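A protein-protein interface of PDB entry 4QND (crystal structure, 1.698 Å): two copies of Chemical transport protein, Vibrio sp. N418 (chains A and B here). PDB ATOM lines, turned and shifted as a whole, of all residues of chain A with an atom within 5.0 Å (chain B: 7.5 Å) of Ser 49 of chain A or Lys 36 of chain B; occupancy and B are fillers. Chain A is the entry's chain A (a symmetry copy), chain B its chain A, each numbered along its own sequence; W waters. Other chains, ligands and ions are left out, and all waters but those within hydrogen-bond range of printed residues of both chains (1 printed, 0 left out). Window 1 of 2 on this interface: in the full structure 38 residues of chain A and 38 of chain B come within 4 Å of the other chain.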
ATOM      1  N   LEU A  46       0.476  -2.875   4.885  1.00  0.00           N
ATOM      2  CA  LEU A  46       0.391  -2.561   3.460  1.00  0.00           C
ATOM      3  C   LEU A  46       0.815  -3.753   2.604  1.00  0.00           C
ATOM      4  O   LEU A  46       0.534  -3.803   1.406  1.00  0.00           O
ATOM      5  CB  LEU A  46       1.249  -1.337   3.124  1.00  0.00           C
ATOM      6  CG  LEU A  46       0.994  -0.668   1.773  1.00  0.00           C
ATOM      7  CD1 LEU A  46      -0.457  -0.227   1.658  1.00  0.00           C
ATOM      8  CD2 LEU A  46       1.934   0.511   1.568  1.00  0.00           C
ATOM      9  N   GLY A  47       1.488  -4.718   3.226  1.00  0.00           N
ATOM     10  CA  GLY A  47       1.897  -5.931   2.541  1.00  0.00           C
ATOM     11  C   GLY A  47       0.756  -6.922   2.387  1.00  0.00           C
ATOM     12  O   GLY A  47       0.901  -7.945   1.725  1.00  0.00           O
ATOM     13  N   LEU A  48      -0.379  -6.613   3.008  1.00  0.00           N
ATOM     14  CA  LEU A  48      -1.564  -7.459   2.922  1.00  0.00           C
ATOM     15  C   LEU A  48      -2.521  -6.947   1.849  1.00  0.00           C
ATOM     16  O   LEU A  48      -2.724  -5.742   1.712  1.00  0.00           O
ATOM     17  CB  LEU A  48      -2.273  -7.524   4.277  1.00  0.00           C
ATOM     18  CG  LEU A  48      -1.548  -8.271   5.396  1.00  0.00           C
ATOM     19  CD1 LEU A  48      -1.982  -7.746   6.753  1.00  0.00           C
ATOM     20  CD2 LEU A  48      -1.843  -9.755   5.295  1.00  0.00           C
ATOM     21  N   SER A  49      -3.106  -7.863   1.086  1.00  0.00           N
ATOM     22  CA  SER A  49      -4.027  -7.475   0.026  1.00  0.00           C
ATOM     23  C   SER A  49      -5.462  -7.425   0.527  1.00  0.00           C
ATOM     24  O   SER A  49      -6.035  -8.450   0.899  1.00  0.00           O
ATOM     25  CB  SER A  49      -3.930  -8.436  -1.158  1.00  0.00           C
ATOM     26  OG  SER A  49      -4.951  -8.166  -2.100  1.00  0.00           O
ATOM     27  N   LEU A  50      -6.037  -6.227   0.530  1.00  0.00           N
ATOM     28  CA  LEU A  50      -7.427  -6.043   0.922  1.00  0.00           C
ATOM     29  C   LEU A  50      -8.351  -6.834   0.003  1.00  0.00           C
ATOM     30  O   LEU A  50      -9.334  -7.421   0.456  1.00  0.00           O
ATOM     31  CB  LEU A  50      -7.796  -4.558   0.903  1.00  0.00           C
ATOM     32  CG  LEU A  50      -9.232  -4.204   1.289  1.00  0.00           C
ATOM     33  CD1 LEU A  50      -9.545  -4.681   2.700  1.00  0.00           C
ATOM     34  CD2 LEU A  50      -9.469  -2.707   1.159  1.00  0.00           C
ATOM     35  N   THR A  51      -8.019  -6.853  -1.288  1.00  0.00           N
ATOM     36  CA  THR A  51      -8.795  -7.599  -2.279  1.00  0.00           C
ATOM     37  C   THR A  51      -8.905  -9.071  -1.898  1.00  0.00           C
ATOM     38  O   THR A  51      -9.994  -9.656  -1.916  1.00  0.00           O
ATOM     39  CB  THR A  51      -8.166  -7.491  -3.684  1.00  0.00           C
ATOM     40  OG1 THR A  51      -8.115  -6.117  -4.087  1.00  0.00           O
ATOM     41  CG2 THR A  51      -8.975  -8.287  -4.699  1.00  0.00           C
ATOM     42  N   THR A  52      -7.770  -9.665  -1.545  1.00  0.00           N
ATOM     43  CA  THR A  52      -7.718 -11.067  -1.148  1.00  0.00           C
ATOM     44  C   THR A  52      -8.647 -11.374   0.024  1.00  0.00           C
ATOM     45  O   THR A  52      -9.454 -12.296  -0.044  1.00  0.00           O
ATOM     46  CB  THR A  52      -6.282 -11.482  -0.773  1.00  0.00           C
ATOM     47  OG1 THR A  52      -5.442 -11.397  -1.932  1.00  0.00           O
ATOM     48  CG2 THR A  52      -6.261 -12.904  -0.244  1.00  0.00           C
ATOM     49  N   TRP A  53      -8.551 -10.590   1.093  1.00  0.00           N
ATOM     50  CA  TRP A  53      -9.312 -10.904   2.298  1.00  0.00           C
ATOM     51  C   TRP A  53     -10.789 -10.546   2.154  1.00  0.00           C
ATOM     52  O   TRP A  53     -11.642 -11.176   2.776  1.00  0.00           O
ATOM     53  CB  TRP A  53      -8.672 -10.214   3.507  1.00  0.00           C
ATOM     54  CG  TRP A  53      -7.289 -10.757   3.750  1.00  0.00           C
ATOM     55  CD1 TRP A  53      -6.109 -10.201   3.346  1.00  0.00           C
ATOM     56  CD2 TRP A  53      -6.949 -11.991   4.396  1.00  0.00           C
ATOM     57  NE1 TRP A  53      -5.055 -11.000   3.720  1.00  0.00           N
ATOM     58  CE2 TRP A  53      -5.544 -12.106   4.365  1.00  0.00           C
ATOM     59  CE3 TRP A  53      -7.695 -13.004   5.008  1.00  0.00           C
ATOM     60  CZ2 TRP A  53      -4.870 -13.192   4.923  1.00  0.00           C
ATOM     61  CZ3 TRP A  53      -7.023 -14.083   5.561  1.00  0.00           C
ATOM     62  CH2 TRP A  53      -5.626 -14.168   5.516  1.00  0.00           C
ATOM     63  N   ILE A  93      -6.871  -4.230   7.880  1.00  0.00           N
ATOM     64  CA  ILE A  93      -6.098  -3.719   6.750  1.00  0.00           C
ATOM     65  C   ILE A  93      -6.511  -2.283   6.439  1.00  0.00           C
ATOM     66  O   ILE A  93      -5.666  -1.417   6.218  1.00  0.00           O
ATOM     67  CB  ILE A  93      -6.275  -4.609   5.504  1.00  0.00           C
ATOM     68  CG1 ILE A  93      -5.651  -5.984   5.746  1.00  0.00           C
ATOM     69  CG2 ILE A  93      -5.653  -3.953   4.278  1.00  0.00           C
ATOM     70  CD1 ILE A  93      -5.979  -7.005   4.676  1.00  0.00           C
ATOM     71  N   THR A 100      -6.291   0.110   0.517  1.00  0.00           N
ATOM     72  CA  THR A 100      -5.311  -0.420  -0.424  1.00  0.00           C
ATOM     73  C   THR A 100      -5.967  -1.523  -1.245  1.00  0.00           C
ATOM     74  O   THR A 100      -7.151  -1.810  -1.068  1.00  0.00           O
ATOM     75  CB  THR A 100      -4.058  -0.966   0.299  1.00  0.00           C
ATOM     76  OG1 THR A 100      -3.086  -1.391  -0.665  1.00  0.00           O
ATOM     77  CG2 THR A 100      -4.425  -2.138   1.202  1.00  0.00           C
ATOM     78  N   TYR A 101      -5.211  -2.134  -2.150  1.00  0.00           N
ATOM     79  CA  TYR A 101      -5.731  -3.262  -2.920  1.00  0.00           C
ATOM     80  C   TYR A 101      -5.311  -4.587  -2.289  1.00  0.00           C
ATOM     81  O   TYR A 101      -5.613  -5.657  -2.815  1.00  0.00           O
ATOM     82  CB  TYR A 101      -5.262  -3.194  -4.377  1.00  0.00           C
ATOM     83  CG  TYR A 101      -3.765  -3.312  -4.560  1.00  0.00           C
ATOM     84  CD1 TYR A 101      -2.955  -2.185  -4.552  1.00  0.00           C
ATOM     85  CD2 TYR A 101      -3.163  -4.550  -4.747  1.00  0.00           C
ATOM     86  CE1 TYR A 101      -1.586  -2.286  -4.722  1.00  0.00           C
ATOM     87  CE2 TYR A 101      -1.795  -4.663  -4.916  1.00  0.00           C
ATOM     88  CZ  TYR A 101      -1.013  -3.528  -4.903  1.00  0.00           C
ATOM     89  OH  TYR A 101       0.348  -3.632  -5.068  1.00  0.00           O
ATOM     90  N   ALA B  29      -8.194 -15.338  -5.824  1.00  0.00           N
ATOM     91  CA  ALA B  29      -8.174 -14.123  -5.009  1.00  0.00           C
ATOM     92  C   ALA B  29      -6.843 -13.920  -4.294  1.00  0.00           C
ATOM     93  O   ALA B  29      -6.544 -12.822  -3.833  1.00  0.00           O
ATOM     94  CB  ALA B  29      -9.299 -14.157  -3.992  1.00  0.00           C
ATOM     95  N   THR B  30      -6.053 -14.983  -4.184  1.00  0.00           N
ATOM     96  CA  THR B  30      -4.776 -14.913  -3.483  1.00  0.00           C
ATOM     97  C   THR B  30      -3.701 -14.271  -4.366  1.00  0.00           C
ATOM     98  O   THR B  30      -2.645 -13.866  -3.879  1.00  0.00           O
ATOM     99  CB  THR B  30      -4.321 -16.318  -3.023  1.00  0.00           C
ATOM    100  OG1 THR B  30      -5.403 -16.970  -2.342  1.00  0.00           O
ATOM    101  CG2 THR B  30      -3.127 -16.238  -2.080  1.00  0.00           C
ATOM    102  N   MET B  31      -3.979 -14.155  -5.661  1.00  0.00           N
ATOM    103  CA  MET B  31      -3.005 -13.589  -6.594  1.00  0.00           C
ATOM    104  C   MET B  31      -2.571 -12.145  -6.249  1.00  0.00           C
ATOM    105  O   MET B  31      -1.378 -11.848  -6.298  1.00  0.00           O
ATOM    106  CB  MET B  31      -3.545 -13.667  -8.031  1.00  0.00           C
ATOM    107  CG  MET B  31      -3.606 -15.093  -8.575  1.00  0.00           C
ATOM    108  SD  MET B  31      -3.848 -15.201 -10.365  1.00  0.00           S
ATOM    109  CE  MET B  31      -5.472 -14.462 -10.545  1.00  0.00           C
ATOM    110  N   PRO B  32      -3.517 -11.249  -5.890  1.00  0.00           N
ATOM    111  CA  PRO B  32      -3.047  -9.925  -5.452  1.00  0.00           C
ATOM    112  C   PRO B  32      -2.198  -9.975  -4.182  1.00  0.00           C
ATOM    113  O   PRO B  32      -1.330  -9.125  -3.987  1.00  0.00           O
ATOM    114  CB  PRO B  32      -4.345  -9.157  -5.182  1.00  0.00           C
ATOM    115  CG  PRO B  32      -5.372  -9.843  -5.981  1.00  0.00           C
ATOM    116  CD  PRO B  32      -4.985 -11.286  -6.023  1.00  0.00           C
ATOM    117  N   GLN B  33      -2.457 -10.954  -3.321  1.00  0.00           N
ATOM    118  CA  GLN B  33      -1.655 -11.118  -2.113  1.00  0.00           C
ATOM    119  C   GLN B  33      -0.257 -11.597  -2.478  1.00  0.00           C
ATOM    120  O   GLN B  33       0.728 -11.169  -1.884  1.00  0.00           O
ATOM    121  CB  GLN B  33      -2.319 -12.098  -1.142  1.00  0.00           C
ATOM    122  CG  GLN B  33      -1.542 -12.318   0.152  1.00  0.00           C
ATOM    123  CD  GLN B  33      -1.358 -11.040   0.950  1.00  0.00           C
ATOM    124  OE1 GLN B  33      -2.249 -10.622   1.691  1.00  0.00           O
ATOM    125  NE2 GLN B  33      -0.195 -10.412   0.802  1.00  0.00           N
ATOM    126  N   LEU B  34      -0.176 -12.492  -3.460  1.00  0.00           N
ATOM    127  CA  LEU B  34       1.114 -12.967  -3.948  1.00  0.00           C
ATOM    128  C   LEU B  34       1.872 -11.839  -4.639  1.00  0.00           C
ATOM    129  O   LEU B  34       3.098 -11.742  -4.533  1.00  0.00           O
ATOM    130  CB  LEU B  34       0.921 -14.150  -4.898  1.00  0.00           C
ATOM    131  CG  LEU B  34       0.645 -15.480  -4.194  1.00  0.00           C
ATOM    132  CD1 LEU B  34      -0.051 -16.447  -5.135  1.00  0.00           C
ATOM    133  CD2 LEU B  34       1.944 -16.078  -3.680  1.00  0.00           C
ATOM    134  N   TYR B  35       1.134 -10.984  -5.338  1.00  0.00           N
ATOM    135  CA  TYR B  35       1.729  -9.838  -6.014  1.00  0.00           C
ATOM    136  C   TYR B  35       2.377  -8.890  -5.009  1.00  0.00           C
ATOM    137  O   TYR B  35       3.485  -8.405  -5.229  1.00  0.00           O
ATOM    138  CB  TYR B  35       0.676  -9.099  -6.839  1.00  0.00           C
ATOM    139  CG  TYR B  35       1.238  -7.940  -7.631  1.00  0.00           C
ATOM    140  CD1 TYR B  35       1.148  -6.639  -7.154  1.00  0.00           C
ATOM    141  CD2 TYR B  35       1.859  -8.149  -8.855  1.00  0.00           C
ATOM    142  CE1 TYR B  35       1.663  -5.579  -7.871  1.00  0.00           C
ATOM    143  CE2 TYR B  35       2.377  -7.092  -9.582  1.00  0.00           C
ATOM    144  CZ  TYR B  35       2.276  -5.810  -9.084  1.00  0.00           C
ATOM    145  OH  TYR B  35       2.788  -4.755  -9.802  1.00  0.00           O
ATOM    146  N   LYS B  36       1.687  -8.632  -3.903  1.00  0.00           N
ATOM    147  CA  LYS B  36       2.239  -7.769  -2.861  1.00  0.00           C
ATOM    148  C   LYS B  36       3.470  -8.392  -2.211  1.00  0.00           C
ATOM    149  O   LYS B  36       4.449  -7.703  -1.942  1.00  0.00           O
ATOM    150  CB  LYS B  36       1.184  -7.461  -1.794  1.00  0.00           C
ATOM    151  CG  LYS B  36       0.168  -6.409  -2.208  1.00  0.00           C
ATOM    152  CD  LYS B  36      -0.510  -5.791  -0.994  1.00  0.00           C
ATOM    153  CE  LYS B  36      -1.349  -4.580  -1.382  1.00  0.00           C
ATOM    154  NZ  LYS B  36      -1.853  -3.843  -0.187  1.00  0.00           N
ATOM    155  N   LEU B  37       3.419  -9.697  -1.966  1.00  0.00           N
ATOM    156  CA  LEU B  37       4.518 -10.403  -1.313  1.00  0.00           C
ATOM    157  C   LEU B  37       5.784 -10.434  -2.171  1.00  0.00           C
ATOM    158  O   LEU B  37       6.888 -10.226  -1.671  1.00  0.00           O
ATOM    159  CB  LEU B  37       4.094 -11.837  -0.961  1.00  0.00           C
ATOM    160  CG  LEU B  37       5.198 -12.800  -0.513  1.00  0.00           C
ATOM    161  CD1 LEU B  37       5.884 -12.313   0.759  1.00  0.00           C
ATOM    162  CD2 LEU B  37       4.636 -14.204  -0.313  1.00  0.00           C
ATOM    163  N   TYR B  38       5.619 -10.688  -3.463  1.00  0.00           N
ATOM    164  CA  TYR B  38       6.761 -10.904  -4.344  1.00  0.00           C
ATOM    165  C   TYR B  38       7.188  -9.667  -5.126  1.00  0.00           C
ATOM    166  O   TYR B  38       8.368  -9.503  -5.433  1.00  0.00           O
ATOM    167  CB  TYR B  38       6.456 -12.026  -5.335  1.00  0.00           C
ATOM    168  CG  TYR B  38       6.613 -13.427  -4.784  1.00  0.00           C
ATOM    169  CD1 TYR B  38       7.873 -13.973  -4.570  1.00  0.00           C
ATOM    170  CD2 TYR B  38       5.504 -14.214  -4.505  1.00  0.00           C
ATOM    171  CE1 TYR B  38       8.023 -15.259  -4.084  1.00  0.00           C
ATOM    172  CE2 TYR B  38       5.643 -15.501  -4.016  1.00  0.00           C
ATOM    173  CZ  TYR B  38       6.906 -16.018  -3.809  1.00  0.00           C
ATOM    174  OH  TYR B  38       7.050 -17.299  -3.322  1.00  0.00           O
ATOM    175  N   VAL B  39       6.232  -8.809  -5.465  1.00  0.00           N
ATOM    176  CA  VAL B  39       6.501  -7.739  -6.418  1.00  0.00           C
ATOM    177  C   VAL B  39       6.457  -6.339  -5.809  1.00  0.00           C
ATOM    178  O   VAL B  39       7.465  -5.632  -5.802  1.00  0.00           O
ATOM    179  CB  VAL B  39       5.505  -7.796  -7.595  1.00  0.00           C
ATOM    180  CG1 VAL B  39       5.851  -6.749  -8.645  1.00  0.00           C
ATOM    181  CG2 VAL B  39       5.489  -9.191  -8.207  1.00  0.00           C
ATOM    182  N   SER B  40       5.298  -5.940  -5.296  1.00  0.00           N
ATOM    183  CA  SER B  40       5.083  -4.538  -4.937  1.00  0.00           C
ATOM    184  C   SER B  40       5.454  -4.170  -3.501  1.00  0.00           C
ATOM    185  O   SER B  40       5.888  -3.046  -3.249  1.00  0.00           O
ATOM    186  CB  SER B  40       3.621  -4.157  -5.197  1.00  0.00           C
ATOM    187  OG  SER B  40       2.735  -4.952  -4.432  1.00  0.00           O
ATOM    188  N   HIS B  41       5.283  -5.098  -2.562  1.00  0.00           N
ATOM    189  CA  HIS B  41       5.513  -4.780  -1.149  1.00  0.00           C
ATOM    190  C   HIS B  41       6.246  -5.866  -0.368  1.00  0.00           C
ATOM    191  O   HIS B  41       5.855  -6.196   0.754  1.00  0.00           O
ATOM    192  CB  HIS B  41       4.182  -4.479  -0.451  1.00  0.00           C
ATOM    193  CG  HIS B  41       3.533  -3.209  -0.912  1.00  0.00           C
ATOM    194  ND1 HIS B  41       2.546  -3.186  -1.866  1.00  0.00           N
ATOM    195  CD2 HIS B  41       3.746  -1.924  -0.544  1.00  0.00           C
ATOM    196  CE1 HIS B  41       2.168  -1.932  -2.070  1.00  0.00           C
ATOM    197  NE2 HIS B  41       2.879  -1.151  -1.283  1.00  0.00           N
ATOM    198  N   SER B  42       7.317  -6.401  -0.947  1.00  0.00           N
ATOM    199  CA  SER B  42       8.118  -7.424  -0.280  1.00  0.00           C
ATOM    200  C   SER B  42       8.700  -6.930   1.045  1.00  0.00           C
ATOM    201  O   SER B  42       8.953  -7.720   1.952  1.00  0.00           O
ATOM    202  CB  SER B  42       9.252  -7.896  -1.192  1.00  0.00           C
ATOM    203  OG  SER B  42       8.754  -8.462  -2.390  1.00  0.00           O
ATOM    204  N   GLU B  43       8.903  -5.620   1.158  1.00  0.00           N
ATOM    205  CA  GLU B  43       9.474  -5.046   2.373  1.00  0.00           C
ATOM    206  C   GLU B  43       8.516  -5.163   3.557  1.00  0.00           C
ATOM    207  O   GLU B  43       8.892  -4.896   4.695  1.00  0.00           O
ATOM    208  CB  GLU B  43       9.859  -3.578   2.149  1.00  0.00           C
ATOM    209  CG  GLU B  43       8.679  -2.616   2.056  1.00  0.00           C
ATOM    210  CD  GLU B  43       8.049  -2.570   0.677  1.00  0.00           C
ATOM    211  OE1 GLU B  43       8.467  -3.350  -0.202  1.00  0.00           O
ATOM    212  OE2 GLU B  43       7.126  -1.752   0.475  1.00  0.00           O
ATOM    213  N   HIS B  44       7.278  -5.570   3.288  1.00  0.00           N
ATOM    214  CA  HIS B  44       6.287  -5.745   4.346  1.00  0.00           C
ATOM    215  C   HIS B  44       5.930  -7.217   4.559  1.00  0.00           C
ATOM    216  O   HIS B  44       4.908  -7.528   5.172  1.00  0.00           O
ATOM    217  CB  HIS B  44       5.027  -4.936   4.025  1.00  0.00           C
ATOM    218  CG  HIS B  44       5.234  -3.450   4.072  1.00  0.00           C
ATOM    219  ND1 HIS B  44       4.806  -2.608   3.073  1.00  0.00           N
ATOM    220  CD2 HIS B  44       5.818  -2.666   5.009  1.00  0.00           C
ATOM    221  CE1 HIS B  44       5.124  -1.360   3.387  1.00  0.00           C
ATOM    222  NE2 HIS B  44       5.735  -1.371   4.553  1.00  0.00           N
ATOM    223  N   ALA B  45       6.778  -8.117   4.069  1.00  0.00           N
ATOM    224  CA  ALA B  45       6.525  -9.555   4.179  1.00  0.00           C
ATOM    225  C   ALA B  45       6.472 -10.037   5.629  1.00  0.00           C
ATOM    226  O   ALA B  45       5.831 -11.047   5.928  1.00  0.00           O
ATOM    227  CB  ALA B  45       7.582 -10.333   3.411  1.00  0.00           C
ATOM    228  N   LEU B  48       3.208 -10.812   7.282  1.00  0.00           N
ATOM    229  CA  LEU B  48       2.500 -12.036   6.922  1.00  0.00           C
ATOM    230  C   LEU B  48       2.881 -13.179   7.859  1.00  0.00           C
ATOM    231  O   LEU B  48       4.046 -13.332   8.222  1.00  0.00           O
ATOM    232  CB  LEU B  48       2.800 -12.419   5.471  1.00  0.00           C
ATOM    233  CG  LEU B  48       2.226 -11.505   4.387  1.00  0.00           C
ATOM    234  CD1 LEU B  48       3.069 -11.584   3.127  1.00  0.00           C
ATOM    235  CD2 LEU B  48       0.797 -11.908   4.083  1.00  0.00           C
ATOM    236  N   MET B  89       2.874 -18.676  -1.214  1.00  0.00           N
ATOM    237  CA  MET B  89       2.903 -17.715  -0.111  1.00  0.00           C
ATOM    238  C   MET B  89       3.956 -18.116   0.921  1.00  0.00           C
ATOM    239  O   MET B  89       4.730 -17.281   1.379  1.00  0.00           O
ATOM    240  CB  MET B  89       1.529 -17.601   0.557  1.00  0.00           C
ATOM    241  CG  MET B  89       0.498 -16.794  -0.226  1.00  0.00           C
ATOM    242  SD  MET B  89       0.972 -15.063  -0.457  1.00  0.00           S
ATOM    243  CE  MET B  89       1.101 -14.523   1.249  1.00  0.00           C
ATOM    244  N   HIS B  96      11.651 -13.685   1.861  1.00  0.00           N
ATOM    245  CA  HIS B  96      11.801 -12.263   2.159  1.00  0.00           C
ATOM    246  C   HIS B  96      11.887 -11.941   3.654  1.00  0.00           C
ATOM    247  O   HIS B  96      12.014 -10.777   4.028  1.00  0.00           O
ATOM    248  CB  HIS B  96      10.653 -11.472   1.526  1.00  0.00           C
ATOM    249  CG  HIS B  96      10.704 -11.431   0.031  1.00  0.00           C
ATOM    250  ND1 HIS B  96      11.586 -10.630  -0.663  1.00  0.00           N
ATOM    251  CD2 HIS B  96       9.986 -12.095  -0.907  1.00  0.00           C
ATOM    252  CE1 HIS B  96      11.408 -10.799  -1.959  1.00  0.00           C
ATOM    253  NE2 HIS B  96      10.443 -11.685  -2.134  1.00  0.00           N
HETATM  254  O   HOH W   1       4.035  -8.355   1.560  1.00  0.00           O
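O of Ala 29 of chain B lies within hydrogen-bond range of OG1 of Thr 52 of chain A (2.6 Å). The backbone carbonyl oxygen of Gly 47 of chain A is in hydrogen-bond range of the side-chain amide nitrogen of Gln 33 of chain B (2.9 Å). The backbone NH of Ser 49 of chain A sits at hydrogen-bond distance from the side-chain amide oxygen of Gln 33 of chain B (3.0 Å). The backbone NH (N) of Gln 33 of chain B lies close to the side-chain hydroxyl (OG1) of Thr 52 of chain A (3.3 Å). The side-chain amide oxygen of Gln 33 of chain B lies within hydrogen-bond range of the indole nitrogen of Trp 53 of chain A, 3.5 Å away. O of Leu 46 of chain A lies within hydrogen-bond range of NZ of Lys 36 of chain B, 2.9 Å away. The side-chain amino group (NZ) of Lys 36 of chain B is in hydrogen-bond range of the backbone carbonyl oxygen (O) of Leu 48 of chain A, at 2.8 Å. NZ of Lys 36 of chain B lies within hydrogen-bond range of OG1 of Thr 100 of chain A (2.8 Å). OG of Ser 40 of chain B lies within hydrogen-bond range of OH of Tyr 101 of chain A (2.8 Å).
Leu 48 of chain A touches its own counterpart, Leu 48 of chain B. 1 position is printed for both chains. Of the 21 pairs that touch across the chains among the printed residues, 1 has its exchanged pair printed and touching as well.
Of the 20 printed residues of chain B, 10 touch a printed residue of chain A. Hydrophobic or aromatic side chains of chain B that line the printed part of chain A: Pro 32, Tyr 35, His 41, His 44 and Leu 48. Printed residues of chain A that touch a printed residue of chain B: Leu 46, Gly 47, Leu 48, Ser 49, Thr 52, Trp 53, Thr 100 and Tyr 101. Among the printed residues, no Asp or Glu carboxylate lies within 4 Å of a Lys or Arg side-chain nitrogen of the other chain.
His 41 of chain B touches Leu 46 of chain A (NE2 to CD2, 3.4 Å). Leu 46 of chain A touches His 44 of chain B. O of Gly 47 of chain A touches CB of Lys 36 of chain B, 3.6 Å away. CA of Gly 47 of chain A touches CB of His 44 of chain B, 3.6 Å away. CA of Leu 48 of chain A touches OE1 of Gln 33 of chain B, at 3.5 Å. Leu 48 of chain B touches Leu 48 of chain A (CD2 to CD2, 3.6 Å). Lys 36 of chain B touches Ser 49 of chain A (CD to N, 3.9 Å). Thr 52 of chain A touches Thr 30 of chain B (OG1 to CA, 3.9 Å). Lys 36 of chain B touches Tyr 101 of chain A. His 41 of chain B touches Tyr 101 of chain A (CE1 to OH, 3.9 Å).
Water W1 bridges O of His 41 of chain B (2.9 Å) and O of Gly 47 of chain A (3.2 Å).
Ser 49 of chain A touches just these residues of chain B: Pro 32, Gln 33 and Lys 36. Lys 36 of chain B touches just these residues of chain A: Leu 46 (2.9 Å), Gly 47 (3.6 Å), Leu 48 (2.8 Å), Ser 49 (3.9 Å), Thr 100 (2.8 Å) and Tyr 101 (3.6 Å). Printed residues of chain A within 4 Å of His 44 of chain B: Leu 46 and Gly 47. Of the printed residues of chain B, Leu 46 of chain A touches Lys 36 (2.9 Å), His 41 (3.4 Å) and His 44 (3.8 Å). Printed residues of chain A within 4 Å of Thr 30 of chain B: Thr 52 (3.9 Å). Printed residues of chain B within 4 Å of Thr 52 of chain A: Ala 29 (2.6 Å), Thr 30 (3.9 Å) and Gln 33 (3.3 Å). His 96 of chain B touches none of the printed residues of chain A. The nearest residue of chain A that does not touch Lys 36 of chain B is Leu 50 of chain A (4.9 Å). The nearest printed residue of chain A that does not touch Gln 33 of chain B is Leu 50 of chain A (5.9 Å).
The backbone carbonyl oxygen (O) of Lys 36 of chain B is in hydrogen-bond range of the backbone NH (N) of His 41 of chain B, 2.8 Å away. The backbone NH of Ser 42 of chain B is in hydrogen-bond range of the backbone carbonyl oxygen of Lys 36 of chain B (3.3 Å). The side-chain hydroxyl (OG) of Ser 40 of chain B is in hydrogen-bond range of a ring nitrogen (ND1) of His 41 of chain B. The side-chain hydroxyl (OG) of Ser 49 of chain A sits close to the backbone NH (N) of Thr 51 of chain A. The backbone NH (N) of Thr 52 of chain A lies within hydrogen-bond range of the side-chain hydroxyl (OG) of Ser 49 of chain A. OG1 of Thr 51 of chain A is in hydrogen-bond range of O of Tyr 101 of chain A (2.8 Å).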
